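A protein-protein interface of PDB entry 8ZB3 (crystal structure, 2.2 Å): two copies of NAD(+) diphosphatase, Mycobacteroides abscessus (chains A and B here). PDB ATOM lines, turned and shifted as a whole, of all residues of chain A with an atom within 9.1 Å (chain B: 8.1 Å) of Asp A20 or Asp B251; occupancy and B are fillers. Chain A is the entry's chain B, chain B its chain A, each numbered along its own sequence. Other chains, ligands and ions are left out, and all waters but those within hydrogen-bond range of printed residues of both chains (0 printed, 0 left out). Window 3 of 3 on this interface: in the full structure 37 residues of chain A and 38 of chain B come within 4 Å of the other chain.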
ATOM      1  N   LEU A  16      24.907  -1.616  -5.833  1.00  0.00           N
ATOM      2  CA  LEU A  16      23.698  -1.664  -6.648  1.00  0.00           C
ATOM      3  C   LEU A  16      23.968  -1.118  -8.046  1.00  0.00           C
ATOM      4  O   LEU A  16      24.802  -0.251  -8.213  1.00  0.00           O
ATOM      5  CB  LEU A  16      22.631  -0.802  -5.974  1.00  0.00           C
ATOM      6  CG  LEU A  16      21.278  -0.705  -6.688  1.00  0.00           C
ATOM      7  CD1 LEU A  16      20.403  -1.915  -6.403  1.00  0.00           C
ATOM      8  CD2 LEU A  16      20.561   0.574  -6.299  1.00  0.00           C
ATOM      9  N   ASP A  17      23.173  -1.555  -9.022  1.00  0.00           N
ATOM     10  CA  ASP A  17      23.247  -0.998 -10.363  1.00  0.00           C
ATOM     11  C   ASP A  17      22.463   0.316 -10.414  1.00  0.00           C
ATOM     12  O   ASP A  17      21.242   0.313 -10.537  1.00  0.00           O
ATOM     13  CB  ASP A  17      22.727  -2.005 -11.386  1.00  0.00           C
ATOM     14  CG  ASP A  17      22.704  -1.471 -12.810  1.00  0.00           C
ATOM     15  OD1 ASP A  17      23.391  -0.472 -13.080  1.00  0.00           O
ATOM     16  OD2 ASP A  17      21.966  -2.044 -13.628  1.00  0.00           O
ATOM     17  N   ARG A  18      23.174   1.445 -10.340  1.00  0.00           N
ATOM     18  CA  ARG A  18      22.520   2.733 -10.188  1.00  0.00           C
ATOM     19  C   ARG A  18      21.960   3.240 -11.511  1.00  0.00           C
ATOM     20  O   ARG A  18      21.159   4.176 -11.504  1.00  0.00           O
ATOM     21  CB  ARG A  18      23.471   3.758  -9.572  1.00  0.00           C
ATOM     22  CG  ARG A  18      23.806   3.438  -8.117  1.00  0.00           C
ATOM     23  CD  ARG A  18      24.403   4.601  -7.404  1.00  0.00           C
ATOM     24  NE  ARG A  18      24.565   4.262  -6.014  1.00  0.00           N
ATOM     25  CZ  ARG A  18      24.710   5.139  -5.042  1.00  0.00           C
ATOM     26  NH1 ARG A  18      24.735   6.448  -5.277  1.00  0.00           N
ATOM     27  NH2 ARG A  18      24.719   4.707  -3.798  1.00  0.00           N
ATOM     28  N   ALA A  19      22.398   2.649 -12.633  1.00  0.00           N
ATOM     29  CA  ALA A  19      21.903   3.013 -13.953  1.00  0.00           C
ATOM     30  C   ALA A  19      21.973   4.527 -14.151  1.00  0.00           C
ATOM     31  O   ALA A  19      20.976   5.193 -14.452  1.00  0.00           O
ATOM     32  CB  ALA A  19      20.498   2.503 -14.107  1.00  0.00           C
ATOM     33  N   ASP A  20      23.184   5.058 -13.988  1.00  0.00           N
ATOM     34  CA  ASP A  20      23.456   6.484 -14.062  1.00  0.00           C
ATOM     35  C   ASP A  20      22.946   7.045 -15.387  1.00  0.00           C
ATOM     36  O   ASP A  20      22.349   8.124 -15.426  1.00  0.00           O
ATOM     37  CB  ASP A  20      24.956   6.734 -13.864  1.00  0.00           C
ATOM     38  CG  ASP A  20      25.804   6.189 -15.009  1.00  0.00           C
ATOM     39  OD1 ASP A  20      25.784   4.942 -15.213  1.00  0.00           O
ATOM     40  OD2 ASP A  20      26.478   7.010 -15.716  1.00  0.00           O
ATOM     41  N   GLU A  21      23.126   6.278 -16.468  1.00  0.00           N
ATOM     42  CA  GLU A  21      22.789   6.728 -17.810  1.00  0.00           C
ATOM     43  C   GLU A  21      21.298   7.041 -17.930  1.00  0.00           C
ATOM     44  O   GLU A  21      20.906   7.841 -18.768  1.00  0.00           O
ATOM     45  CB  GLU A  21      23.239   5.685 -18.843  1.00  0.00           C
ATOM     46  CG  GLU A  21      22.486   4.355 -18.799  1.00  0.00           C
ATOM     47  CD  GLU A  21      22.897   3.353 -17.727  1.00  0.00           C
ATOM     48  OE1 GLU A  21      22.360   2.246 -17.756  1.00  0.00           O
ATOM     49  OE2 GLU A  21      23.745   3.685 -16.867  1.00  0.00           O
ATOM     50  N   LEU A  22      20.452   6.436 -17.092  1.00  0.00           N
ATOM     51  CA  LEU A  22      19.018   6.675 -17.195  1.00  0.00           C
ATOM     52  C   LEU A  22      18.606   7.996 -16.543  1.00  0.00           C
ATOM     53  O   LEU A  22      17.498   8.473 -16.791  1.00  0.00           O
ATOM     54  CB  LEU A  22      18.273   5.490 -16.586  1.00  0.00           C
ATOM     55  CG  LEU A  22      18.418   4.164 -17.343  1.00  0.00           C
ATOM     56  CD1 LEU A  22      17.482   3.107 -16.764  1.00  0.00           C
ATOM     57  CD2 LEU A  22      18.166   4.334 -18.844  1.00  0.00           C
ATOM     58  N   ARG A  23      19.473   8.578 -15.700  1.00  0.00           N
ATOM     59  CA  ARG A  23      19.074   9.727 -14.897  1.00  0.00           C
ATOM     60  C   ARG A  23      18.719  10.934 -15.769  1.00  0.00           C
ATOM     61  O   ARG A  23      17.812  11.693 -15.432  1.00  0.00           O
ATOM     62  CB  ARG A  23      20.196  10.145 -13.945  1.00  0.00           C
ATOM     63  CG  ARG A  23      20.433   9.170 -12.806  1.00  0.00           C
ATOM     64  CD  ARG A  23      21.778   9.411 -12.143  1.00  0.00           C
ATOM     65  NE  ARG A  23      22.010   8.459 -11.072  1.00  0.00           N
ATOM     66  CZ  ARG A  23      23.118   8.396 -10.336  1.00  0.00           C
ATOM     67  NH1 ARG A  23      24.134   9.195 -10.586  1.00  0.00           N
ATOM     68  NH2 ARG A  23      23.222   7.530  -9.351  1.00  0.00           N
ATOM     69  N   SER A  24      19.475  11.098 -16.872  1.00  0.00           N
ATOM     70  CA  SER A  24      19.283  12.193 -17.808  1.00  0.00           C
ATOM     71  C   SER A  24      18.398  11.778 -18.983  1.00  0.00           C
ATOM     72  O   SER A  24      18.363  12.477 -19.995  1.00  0.00           O
ATOM     73  CB  SER A  24      20.609  12.670 -18.318  1.00  0.00           C
ATOM     74  OG  SER A  24      21.420  13.123 -17.253  1.00  0.00           O
ATOM     75  N   ASN A  25      17.695  10.642 -18.867  1.00  0.00           N
ATOM     76  CA  ASN A  25      16.856  10.150 -19.949  1.00  0.00           C
ATOM     77  C   ASN A  25      15.410  10.065 -19.462  1.00  0.00           C
ATOM     78  O   ASN A  25      14.935   8.994 -19.070  1.00  0.00           O
ATOM     79  CB  ASN A  25      17.403   8.815 -20.449  1.00  0.00           C
ATOM     80  CG  ASN A  25      16.665   8.265 -21.657  1.00  0.00           C
ATOM     81  OD1 ASN A  25      15.529   8.646 -21.947  1.00  0.00           O
ATOM     82  ND2 ASN A  25      17.301   7.334 -22.340  1.00  0.00           N
ATOM     83  N   LEU A  29      12.963   6.760 -17.998  1.00  0.00           N
ATOM     84  CA  LEU A  29      12.493   6.758 -16.620  1.00  0.00           C
ATOM     85  C   LEU A  29      10.968   6.651 -16.607  1.00  0.00           C
ATOM     86  O   LEU A  29      10.416   5.900 -15.807  1.00  0.00           O
ATOM     87  CB  LEU A  29      12.977   8.023 -15.899  1.00  0.00           C
ATOM     88  CG  LEU A  29      14.485   8.131 -15.649  1.00  0.00           C
ATOM     89  CD1 LEU A  29      14.826   9.446 -14.953  1.00  0.00           C
ATOM     90  CD2 LEU A  29      14.997   6.952 -14.839  1.00  0.00           C
ATOM     91  N   PHE A  72      15.420   8.180  -8.248  1.00  0.00           N
ATOM     92  CA  PHE A  72      15.653   6.955  -8.984  1.00  0.00           C
ATOM     93  C   PHE A  72      16.903   6.260  -8.450  1.00  0.00           C
ATOM     94  O   PHE A  72      18.012   6.781  -8.581  1.00  0.00           O
ATOM     95  CB  PHE A  72      15.778   7.306 -10.471  1.00  0.00           C
ATOM     96  CG  PHE A  72      16.234   6.155 -11.315  1.00  0.00           C
ATOM     97  CD1 PHE A  72      15.422   5.042 -11.497  1.00  0.00           C
ATOM     98  CD2 PHE A  72      17.487   6.157 -11.883  1.00  0.00           C
ATOM     99  CE1 PHE A  72      15.845   3.968 -12.261  1.00  0.00           C
ATOM    100  CE2 PHE A  72      17.905   5.084 -12.656  1.00  0.00           C
ATOM    101  CZ  PHE A  72      17.082   3.996 -12.852  1.00  0.00           C
ATOM    102  N   LEU A  73      16.731   5.074  -7.858  1.00  0.00           N
ATOM    103  CA  LEU A  73      17.824   4.391  -7.185  1.00  0.00           C
ATOM    104  C   LEU A  73      18.600   3.503  -8.153  1.00  0.00           C
ATOM    105  O   LEU A  73      19.735   3.139  -7.873  1.00  0.00           O
ATOM    106  CB  LEU A  73      17.264   3.549  -6.036  1.00  0.00           C
ATOM    107  CG  LEU A  73      16.496   4.311  -4.961  1.00  0.00           C
ATOM    108  CD1 LEU A  73      15.997   3.379  -3.864  1.00  0.00           C
ATOM    109  CD2 LEU A  73      17.354   5.407  -4.342  1.00  0.00           C
ATOM    110  N   GLY A  74      17.975   3.099  -9.259  1.00  0.00           N
ATOM    111  CA  GLY A  74      18.617   2.220 -10.222  1.00  0.00           C
ATOM    112  C   GLY A  74      17.758   0.999 -10.546  1.00  0.00           C
ATOM    113  O   GLY A  74      16.536   1.079 -10.547  1.00  0.00           O
ATOM    114  N   ARG A  75      18.436  -0.117 -10.826  1.00  0.00           N
ATOM    115  CA  ARG A  75      17.799  -1.351 -11.236  1.00  0.00           C
ATOM    116  C   ARG A  75      18.195  -2.455 -10.276  1.00  0.00           C
ATOM    117  O   ARG A  75      19.365  -2.558  -9.928  1.00  0.00           O
ATOM    118  CB  ARG A  75      18.319  -1.829 -12.597  1.00  0.00           C
ATOM    119  CG  ARG A  75      17.988  -0.964 -13.794  1.00  0.00           C
ATOM    120  CD  ARG A  75      18.864  -1.631 -14.865  1.00  0.00           C
ATOM    121  NE  ARG A  75      19.017  -0.793 -16.024  1.00  0.00           N
ATOM    122  CZ  ARG A  75      20.143  -0.242 -16.439  1.00  0.00           C
ATOM    123  NH1 ARG A  75      21.308  -0.540 -15.894  1.00  0.00           N
ATOM    124  NH2 ARG A  75      20.082   0.648 -17.411  1.00  0.00           N
ATOM    125  N   LYS A 141      16.708  15.261 -13.131  1.00  0.00           N
ATOM    126  CA  LYS A 141      17.514  14.095 -13.481  1.00  0.00           C
ATOM    127  C   LYS A 141      17.315  12.976 -12.466  1.00  0.00           C
ATOM    128  O   LYS A 141      18.266  12.459 -11.869  1.00  0.00           O
ATOM    129  CB  LYS A 141      18.978  14.520 -13.590  1.00  0.00           C
ATOM    130  CG  LYS A 141      19.230  15.496 -14.722  1.00  0.00           C
ATOM    131  CD  LYS A 141      20.656  15.938 -14.849  1.00  0.00           C
ATOM    132  CE  LYS A 141      20.864  16.853 -16.034  1.00  0.00           C
ATOM    133  NZ  LYS A 141      22.248  17.366 -16.056  1.00  0.00           N
ATOM    134  N   GLY A 142      16.043  12.599 -12.318  1.00  0.00           N
ATOM    135  CA  GLY A 142      15.663  11.457 -11.510  1.00  0.00           C
ATOM    136  C   GLY A 142      15.959  11.680 -10.035  1.00  0.00           C
ATOM    137  O   GLY A 142      16.058  10.720  -9.301  1.00  0.00           O
ATOM    138  N   TRP A 144      18.720  13.408  -8.935  1.00  0.00           N
ATOM    139  CA  TRP A 144      20.155  13.391  -8.693  1.00  0.00           C
ATOM    140  C   TRP A 144      20.780  14.776  -8.750  1.00  0.00           C
ATOM    141  O   TRP A 144      21.944  14.915  -8.411  1.00  0.00           O
ATOM    142  CB  TRP A 144      20.851  12.386  -9.613  1.00  0.00           C
ATOM    143  CG  TRP A 144      20.493  11.008  -9.147  1.00  0.00           C
ATOM    144  CD1 TRP A 144      19.367  10.309  -9.459  1.00  0.00           C
ATOM    145  CD2 TRP A 144      21.187  10.244  -8.143  1.00  0.00           C
ATOM    146  NE1 TRP A 144      19.347   9.127  -8.767  1.00  0.00           N
ATOM    147  CE2 TRP A 144      20.430   9.072  -7.932  1.00  0.00           C
ATOM    148  CE3 TRP A 144      22.369  10.419  -7.421  1.00  0.00           C
ATOM    149  CZ2 TRP A 144      20.816   8.087  -7.020  1.00  0.00           C
ATOM    150  CZ3 TRP A 144      22.751   9.439  -6.519  1.00  0.00           C
ATOM    151  CH2 TRP A 144      21.972   8.298  -6.306  1.00  0.00           C
ATOM    152  N   GLN B 179      39.464  12.106 -21.776  1.00  0.00           N
ATOM    153  CA  GLN B 179      38.126  12.668 -21.835  1.00  0.00           C
ATOM    154  C   GLN B 179      37.880  13.243 -23.219  1.00  0.00           C
ATOM    155  O   GLN B 179      38.822  13.649 -23.889  1.00  0.00           O
ATOM    156  CB  GLN B 179      37.909  13.733 -20.758  1.00  0.00           C
ATOM    157  CG  GLN B 179      38.008  13.159 -19.343  1.00  0.00           C
ATOM    158  CD  GLN B 179      36.749  12.704 -18.642  1.00  0.00           C
ATOM    159  OE1 GLN B 179      36.520  11.516 -18.417  1.00  0.00           O
ATOM    160  NE2 GLN B 179      35.945  13.659 -18.209  1.00  0.00           N
ATOM    161  N   LYS B 180      36.604  13.284 -23.611  1.00  0.00           N
ATOM    162  CA  LYS B 180      36.198  13.843 -24.889  1.00  0.00           C
ATOM    163  C   LYS B 180      36.733  15.262 -25.097  1.00  0.00           C
ATOM    164  O   LYS B 180      37.166  15.557 -26.208  1.00  0.00           O
ATOM    165  CB  LYS B 180      34.674  13.761 -25.049  1.00  0.00           C
ATOM    166  CG  LYS B 180      34.121  12.345 -25.087  1.00  0.00           C
ATOM    167  CD  LYS B 180      32.783  12.195 -25.802  1.00  0.00           C
ATOM    168  CE  LYS B 180      32.430  10.746 -26.058  1.00  0.00           C
ATOM    169  NZ  LYS B 180      30.984  10.583 -26.326  1.00  0.00           N
ATOM    170  N   ALA B 191      38.346   9.160 -12.667  1.00  0.00           N
ATOM    171  CA  ALA B 191      38.026   9.994 -11.516  1.00  0.00           C
ATOM    172  C   ALA B 191      36.524  10.197 -11.441  1.00  0.00           C
ATOM    173  O   ALA B 191      35.855  10.271 -12.462  1.00  0.00           O
ATOM    174  CB  ALA B 191      38.714  11.329 -11.621  1.00  0.00           C
ATOM    175  N   GLU B 195      29.172   9.409  -4.470  1.00  0.00           N
ATOM    176  CA  GLU B 195      27.744   9.694  -4.362  1.00  0.00           C
ATOM    177  C   GLU B 195      27.245   9.272  -2.984  1.00  0.00           C
ATOM    178  O   GLU B 195      27.893   8.497  -2.267  1.00  0.00           O
ATOM    179  CB  GLU B 195      26.961   8.951  -5.437  1.00  0.00           C
ATOM    180  CG  GLU B 195      27.292   9.410  -6.844  1.00  0.00           C
ATOM    181  CD  GLU B 195      26.388   8.889  -7.953  1.00  0.00           C
ATOM    182  OE1 GLU B 195      26.590   9.341  -9.082  1.00  0.00           O
ATOM    183  OE2 GLU B 195      25.558   7.966  -7.709  1.00  0.00           O
ATOM    184  N   ARG B 206      32.035   1.576  -9.314  1.00  0.00           N
ATOM    185  CA  ARG B 206      30.960   2.162 -10.094  1.00  0.00           C
ATOM    186  C   ARG B 206      31.525   3.112 -11.155  1.00  0.00           C
ATOM    187  O   ARG B 206      31.148   3.027 -12.316  1.00  0.00           O
ATOM    188  CB  ARG B 206      29.949   2.858  -9.178  1.00  0.00           C
ATOM    189  CG  ARG B 206      28.811   3.562  -9.929  1.00  0.00           C
ATOM    190  CD  ARG B 206      27.863   4.363  -9.058  1.00  0.00           C
ATOM    191  NE  ARG B 206      28.542   5.385  -8.262  1.00  0.00           N
ATOM    192  CZ  ARG B 206      29.234   6.421  -8.745  1.00  0.00           C
ATOM    193  NH1 ARG B 206      29.243   6.680 -10.037  1.00  0.00           N
ATOM    194  NH2 ARG B 206      29.891   7.220  -7.920  1.00  0.00           N
ATOM    195  N   GLU B 207      32.432   4.008 -10.766  1.00  0.00           N
ATOM    196  CA  GLU B 207      32.960   5.024 -11.674  1.00  0.00           C
ATOM    197  C   GLU B 207      33.778   4.386 -12.795  1.00  0.00           C
ATOM    198  O   GLU B 207      33.686   4.802 -13.938  1.00  0.00           O
ATOM    199  CB  GLU B 207      33.828   6.042 -10.929  1.00  0.00           C
ATOM    200  CG  GLU B 207      33.047   7.049 -10.121  1.00  0.00           C
ATOM    201  CD  GLU B 207      32.283   8.094 -10.933  1.00  0.00           C
ATOM    202  OE1 GLU B 207      31.407   8.763 -10.346  1.00  0.00           O
ATOM    203  OE2 GLU B 207      32.575   8.245 -12.150  1.00  0.00           O
ATOM    204  N   VAL B 208      34.597   3.395 -12.480  1.00  0.00           N
ATOM    205  CA  VAL B 208      35.355   2.713 -13.512  1.00  0.00           C
ATOM    206  C   VAL B 208      34.394   2.065 -14.519  1.00  0.00           C
ATOM    207  O   VAL B 208      34.585   2.215 -15.723  1.00  0.00           O
ATOM    208  CB  VAL B 208      36.319   1.693 -12.893  1.00  0.00           C
ATOM    209  CG1 VAL B 208      36.907   0.770 -13.937  1.00  0.00           C
ATOM    210  CG2 VAL B 208      37.409   2.410 -12.108  1.00  0.00           C
ATOM    211  N   ALA B 209      33.341   1.393 -14.023  1.00  0.00           N
ATOM    212  CA  ALA B 209      32.341   0.767 -14.877  1.00  0.00           C
ATOM    213  C   ALA B 209      31.665   1.799 -15.774  1.00  0.00           C
ATOM    214  O   ALA B 209      31.560   1.585 -16.976  1.00  0.00           O
ATOM    215  CB  ALA B 209      31.321   0.013 -14.049  1.00  0.00           C
ATOM    216  N   GLU B 210      31.242   2.929 -15.189  1.00  0.00           N
ATOM    217  CA  GLU B 210      30.575   3.983 -15.937  1.00  0.00           C
ATOM    218  C   GLU B 210      31.469   4.547 -17.033  1.00  0.00           C
ATOM    219  O   GLU B 210      30.980   4.882 -18.104  1.00  0.00           O
ATOM    220  CB  GLU B 210      30.171   5.150 -15.039  1.00  0.00           C
ATOM    221  CG  GLU B 210      28.953   4.865 -14.179  1.00  0.00           C
ATOM    222  CD  GLU B 210      28.542   5.999 -13.251  1.00  0.00           C
ATOM    223  OE1 GLU B 210      27.697   5.730 -12.361  1.00  0.00           O
ATOM    224  OE2 GLU B 210      29.065   7.149 -13.433  1.00  0.00           O
ATOM    225  N   GLU B 211      32.768   4.688 -16.769  1.00  0.00           N
ATOM    226  CA  GLU B 211      33.625   5.442 -17.676  1.00  0.00           C
ATOM    227  C   GLU B 211      34.188   4.548 -18.775  1.00  0.00           C
ATOM    228  O   GLU B 211      34.261   4.961 -19.926  1.00  0.00           O
ATOM    229  CB  GLU B 211      34.773   6.115 -16.924  1.00  0.00           C
ATOM    230  CG  GLU B 211      34.290   7.098 -15.875  1.00  0.00           C
ATOM    231  CD  GLU B 211      34.800   8.515 -16.005  1.00  0.00           C
ATOM    232  OE1 GLU B 211      35.356   9.033 -15.014  1.00  0.00           O
ATOM    233  OE2 GLU B 211      34.563   9.102 -17.076  1.00  0.00           O
ATOM    234  N   VAL B 212      34.651   3.351 -18.418  1.00  0.00           N
ATOM    235  CA  VAL B 212      35.335   2.511 -19.385  1.00  0.00           C
ATOM    236  C   VAL B 212      34.798   1.078 -19.370  1.00  0.00           C
ATOM    237  O   VAL B 212      35.378   0.224 -20.040  1.00  0.00           O
ATOM    238  CB  VAL B 212      36.860   2.534 -19.181  1.00  0.00           C
ATOM    239  CG1 VAL B 212      37.406   3.954 -19.241  1.00  0.00           C
ATOM    240  CG2 VAL B 212      37.268   1.827 -17.891  1.00  0.00           C
ATOM    241  N   GLY B 213      33.710   0.824 -18.624  1.00  0.00           N
ATOM    242  CA  GLY B 213      32.968  -0.423 -18.750  1.00  0.00           C
ATOM    243  C   GLY B 213      33.644  -1.624 -18.100  1.00  0.00           C
ATOM    244  O   GLY B 213      33.129  -2.722 -18.209  1.00  0.00           O
ATOM    245  N   ALA B 248      34.049  -0.063 -22.841  1.00  0.00           N
ATOM    246  CA  ALA B 248      32.751   0.412 -23.267  1.00  0.00           C
ATOM    247  C   ALA B 248      32.557   1.802 -22.679  1.00  0.00           C
ATOM    248  O   ALA B 248      32.553   1.956 -21.455  1.00  0.00           O
ATOM    249  CB  ALA B 248      31.678  -0.536 -22.796  1.00  0.00           C
ATOM    250  N   PHE B 249      32.377   2.802 -23.546  1.00  0.00           N
ATOM    251  CA  PHE B 249      32.451   4.193 -23.132  1.00  0.00           C
ATOM    252  C   PHE B 249      31.050   4.717 -22.814  1.00  0.00           C
ATOM    253  O   PHE B 249      30.551   5.641 -23.437  1.00  0.00           O
ATOM    254  CB  PHE B 249      33.333   4.959 -24.119  1.00  0.00           C
ATOM    255  CG  PHE B 249      34.710   4.350 -24.252  1.00  0.00           C
ATOM    256  CD1 PHE B 249      35.489   4.074 -23.138  1.00  0.00           C
ATOM    257  CD2 PHE B 249      35.236   4.041 -25.499  1.00  0.00           C
ATOM    258  CE1 PHE B 249      36.754   3.505 -23.262  1.00  0.00           C
ATOM    259  CE2 PHE B 249      36.493   3.459 -25.622  1.00  0.00           C
ATOM    260  CZ  PHE B 249      37.256   3.195 -24.501  1.00  0.00           C
ATOM    261  N   ASN B 250      30.509   4.166 -21.714  1.00  0.00           N
ATOM    262  CA  ASN B 250      29.079   4.174 -21.414  1.00  0.00           C
ATOM    263  C   ASN B 250      28.564   5.588 -21.178  1.00  0.00           C
ATOM    264  O   ASN B 250      27.742   6.088 -21.947  1.00  0.00           O
ATOM    265  CB  ASN B 250      28.720   3.387 -20.153  1.00  0.00           C
ATOM    266  CG  ASN B 250      28.722   1.879 -20.332  1.00  0.00           C
ATOM    267  OD1 ASN B 250      28.125   1.345 -21.267  1.00  0.00           O
ATOM    268  ND2 ASN B 250      29.374   1.180 -19.420  1.00  0.00           N
ATOM    269  N   ASP B 251      29.027   6.207 -20.083  1.00  0.00           N
ATOM    270  CA  ASP B 251      28.504   7.497 -19.643  1.00  0.00           C
ATOM    271  C   ASP B 251      28.919   8.640 -20.577  1.00  0.00           C
ATOM    272  O   ASP B 251      28.450   9.758 -20.393  1.00  0.00           O
ATOM    273  CB  ASP B 251      28.852   7.815 -18.190  1.00  0.00           C
ATOM    274  CG  ASP B 251      30.315   8.125 -17.891  1.00  0.00           C
ATOM    275  OD1 ASP B 251      31.145   8.142 -18.847  1.00  0.00           O
ATOM    276  OD2 ASP B 251      30.614   8.324 -16.698  1.00  0.00           O
ATOM    277  N   GLY B 252      29.782   8.368 -21.578  1.00  0.00           N
ATOM    278  CA  GLY B 252      30.055   9.309 -22.662  1.00  0.00           C
ATOM    279  C   GLY B 252      31.185  10.303 -22.380  1.00  0.00           C
ATOM    280  O   GLY B 252      31.427  11.219 -23.161  1.00  0.00           O
ATOM    281  N   GLU B 253      31.868  10.134 -21.247  1.00  0.00           N
ATOM    282  CA  GLU B 253      32.816  11.111 -20.744  1.00  0.00           C
ATOM    283  C   GLU B 253      34.214  10.776 -21.282  1.00  0.00           C
ATOM    284  O   GLU B 253      35.018  11.668 -21.525  1.00  0.00           O
ATOM    285  CB  GLU B 253      32.638  11.100 -19.227  1.00  0.00           C
ATOM    286  CG  GLU B 253      33.221  12.281 -18.496  1.00  0.00           C
ATOM    287  CD  GLU B 253      32.567  13.640 -18.683  1.00  0.00           C
ATOM    288  OE1 GLU B 253      31.431  13.754 -19.207  1.00  0.00           O
ATOM    289  OE2 GLU B 253      33.217  14.595 -18.288  1.00  0.00           O
ATOM    290  N   ILE B 254      34.477   9.482 -21.515  1.00  0.00           N
ATOM    291  CA  ILE B 254      35.744   9.020 -22.051  1.00  0.00           C
ATOM    292  C   ILE B 254      35.600   8.813 -23.559  1.00  0.00           C
ATOM    293  O   ILE B 254      34.683   8.133 -24.018  1.00  0.00           O
ATOM    294  CB  ILE B 254      36.219   7.738 -21.334  1.00  0.00           C
ATOM    295  CG1 ILE B 254      36.455   7.968 -19.836  1.00  0.00           C
ATOM    296  CG2 ILE B 254      37.471   7.168 -22.009  1.00  0.00           C
ATOM    297  CD1 ILE B 254      37.617   8.887 -19.511  1.00  0.00           C
ATOM    298  N   ALA B 255      36.544   9.392 -24.316  1.00  0.00           N
ATOM    299  CA  ALA B 255      36.608   9.254 -25.760  1.00  0.00           C
ATOM    300  C   ALA B 255      37.396   8.005 -26.135  1.00  0.00           C
ATOM    301  O   ALA B 255      37.013   7.271 -27.048  1.00  0.00           O
ATOM    302  CB  ALA B 255      37.232  10.491 -26.364  1.00  0.00           C
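The side-chain carboxylate (OE1) of Glu B195 lies within salt-bridge range of the guanidinium group (NH1) of Arg A23 (2.9 Å).
OE2 of Glu B195 is in salt-bridge range of NH1 of Arg A18 (3.0 Å).
The side-chain carboxylate (OE2) of Glu B210 lies close to the side-chain carboxylate (OD2) of Asp A20, at 3.5 Å.
The side-chain carboxylate of Glu B210 lies within salt-bridge range of the guanidinium group of Arg B206 (2.9 Å).
The side-chain carboxylate of Glu B207 lies within salt-bridge range of the guanidinium group of Arg B206, 3.0 Å away.
The backbone carbonyl oxygen (O) of Phe A72 lies within hydrogen-bond range of the indole nitrogen (NE1) of Trp A144 (2.7 Å).
N of Glu B253 lies within hydrogen-bond range of OD1 of Asp B251 (3.2 Å).
OE1 of Glu B195 lies within salt-bridge range of NH1 of Arg B206, at 3.9 Å.
The backbone carbonyl oxygen of Glu B210 is in hydrogen-bond range of the backbone NH of Asp B251, at 3.1 Å.
Arg B206 touches Arg A18 (CD to CD, 3.8 Å).
Asp B251 touches Asp A20.
Trp A144 touches Glu B195.
Of the printed residues of chain B, Asp A20 touches Glu B210 (3.3 Å) and Asp B251 (3.5 Å).
Asp B251 touches one residue of chain A.
Of the printed residues of chain A, Glu B210 touches Asp A20 (3.3 Å).
Of the printed residues of chain B, Trp A144 touches Glu B195.
Of the printed residues of chain A, Glu B195 touches Arg A18 (3.0 Å), Arg A23 (2.9 Å) and Trp A144 (3.4 Å).
Printed residues of chain A within 4 Å of Arg B206: Arg A18 (3.8 Å).
Of the printed residues of chain B, Arg A18 touches Glu B195 (3.0 Å) and Arg B206 (3.8 Å).
The nearest residue of chain B that does not touch Asp A20 is Glu B195 (5.7 Å).
The nearest residue of chain A that does not touch Asp B251 is Glu A21 (5.6 Å).
The nearest printed residue of chain B that does not touch Arg A23 is Glu B210 (5.3 Å).
Of the 18 printed residues of chain A, 4 touch a printed residue of chain B.
Printed residues of chain A that touch a printed residue of chain B: Arg A18, Asp A20, Arg A23 and Trp A144.
Hydrophobic or aromatic side chains of chain A that line the printed part of chain B: Trp A144.
Among the printed residues, 6 pairs touch across the chains.
No position is printed for both chains.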
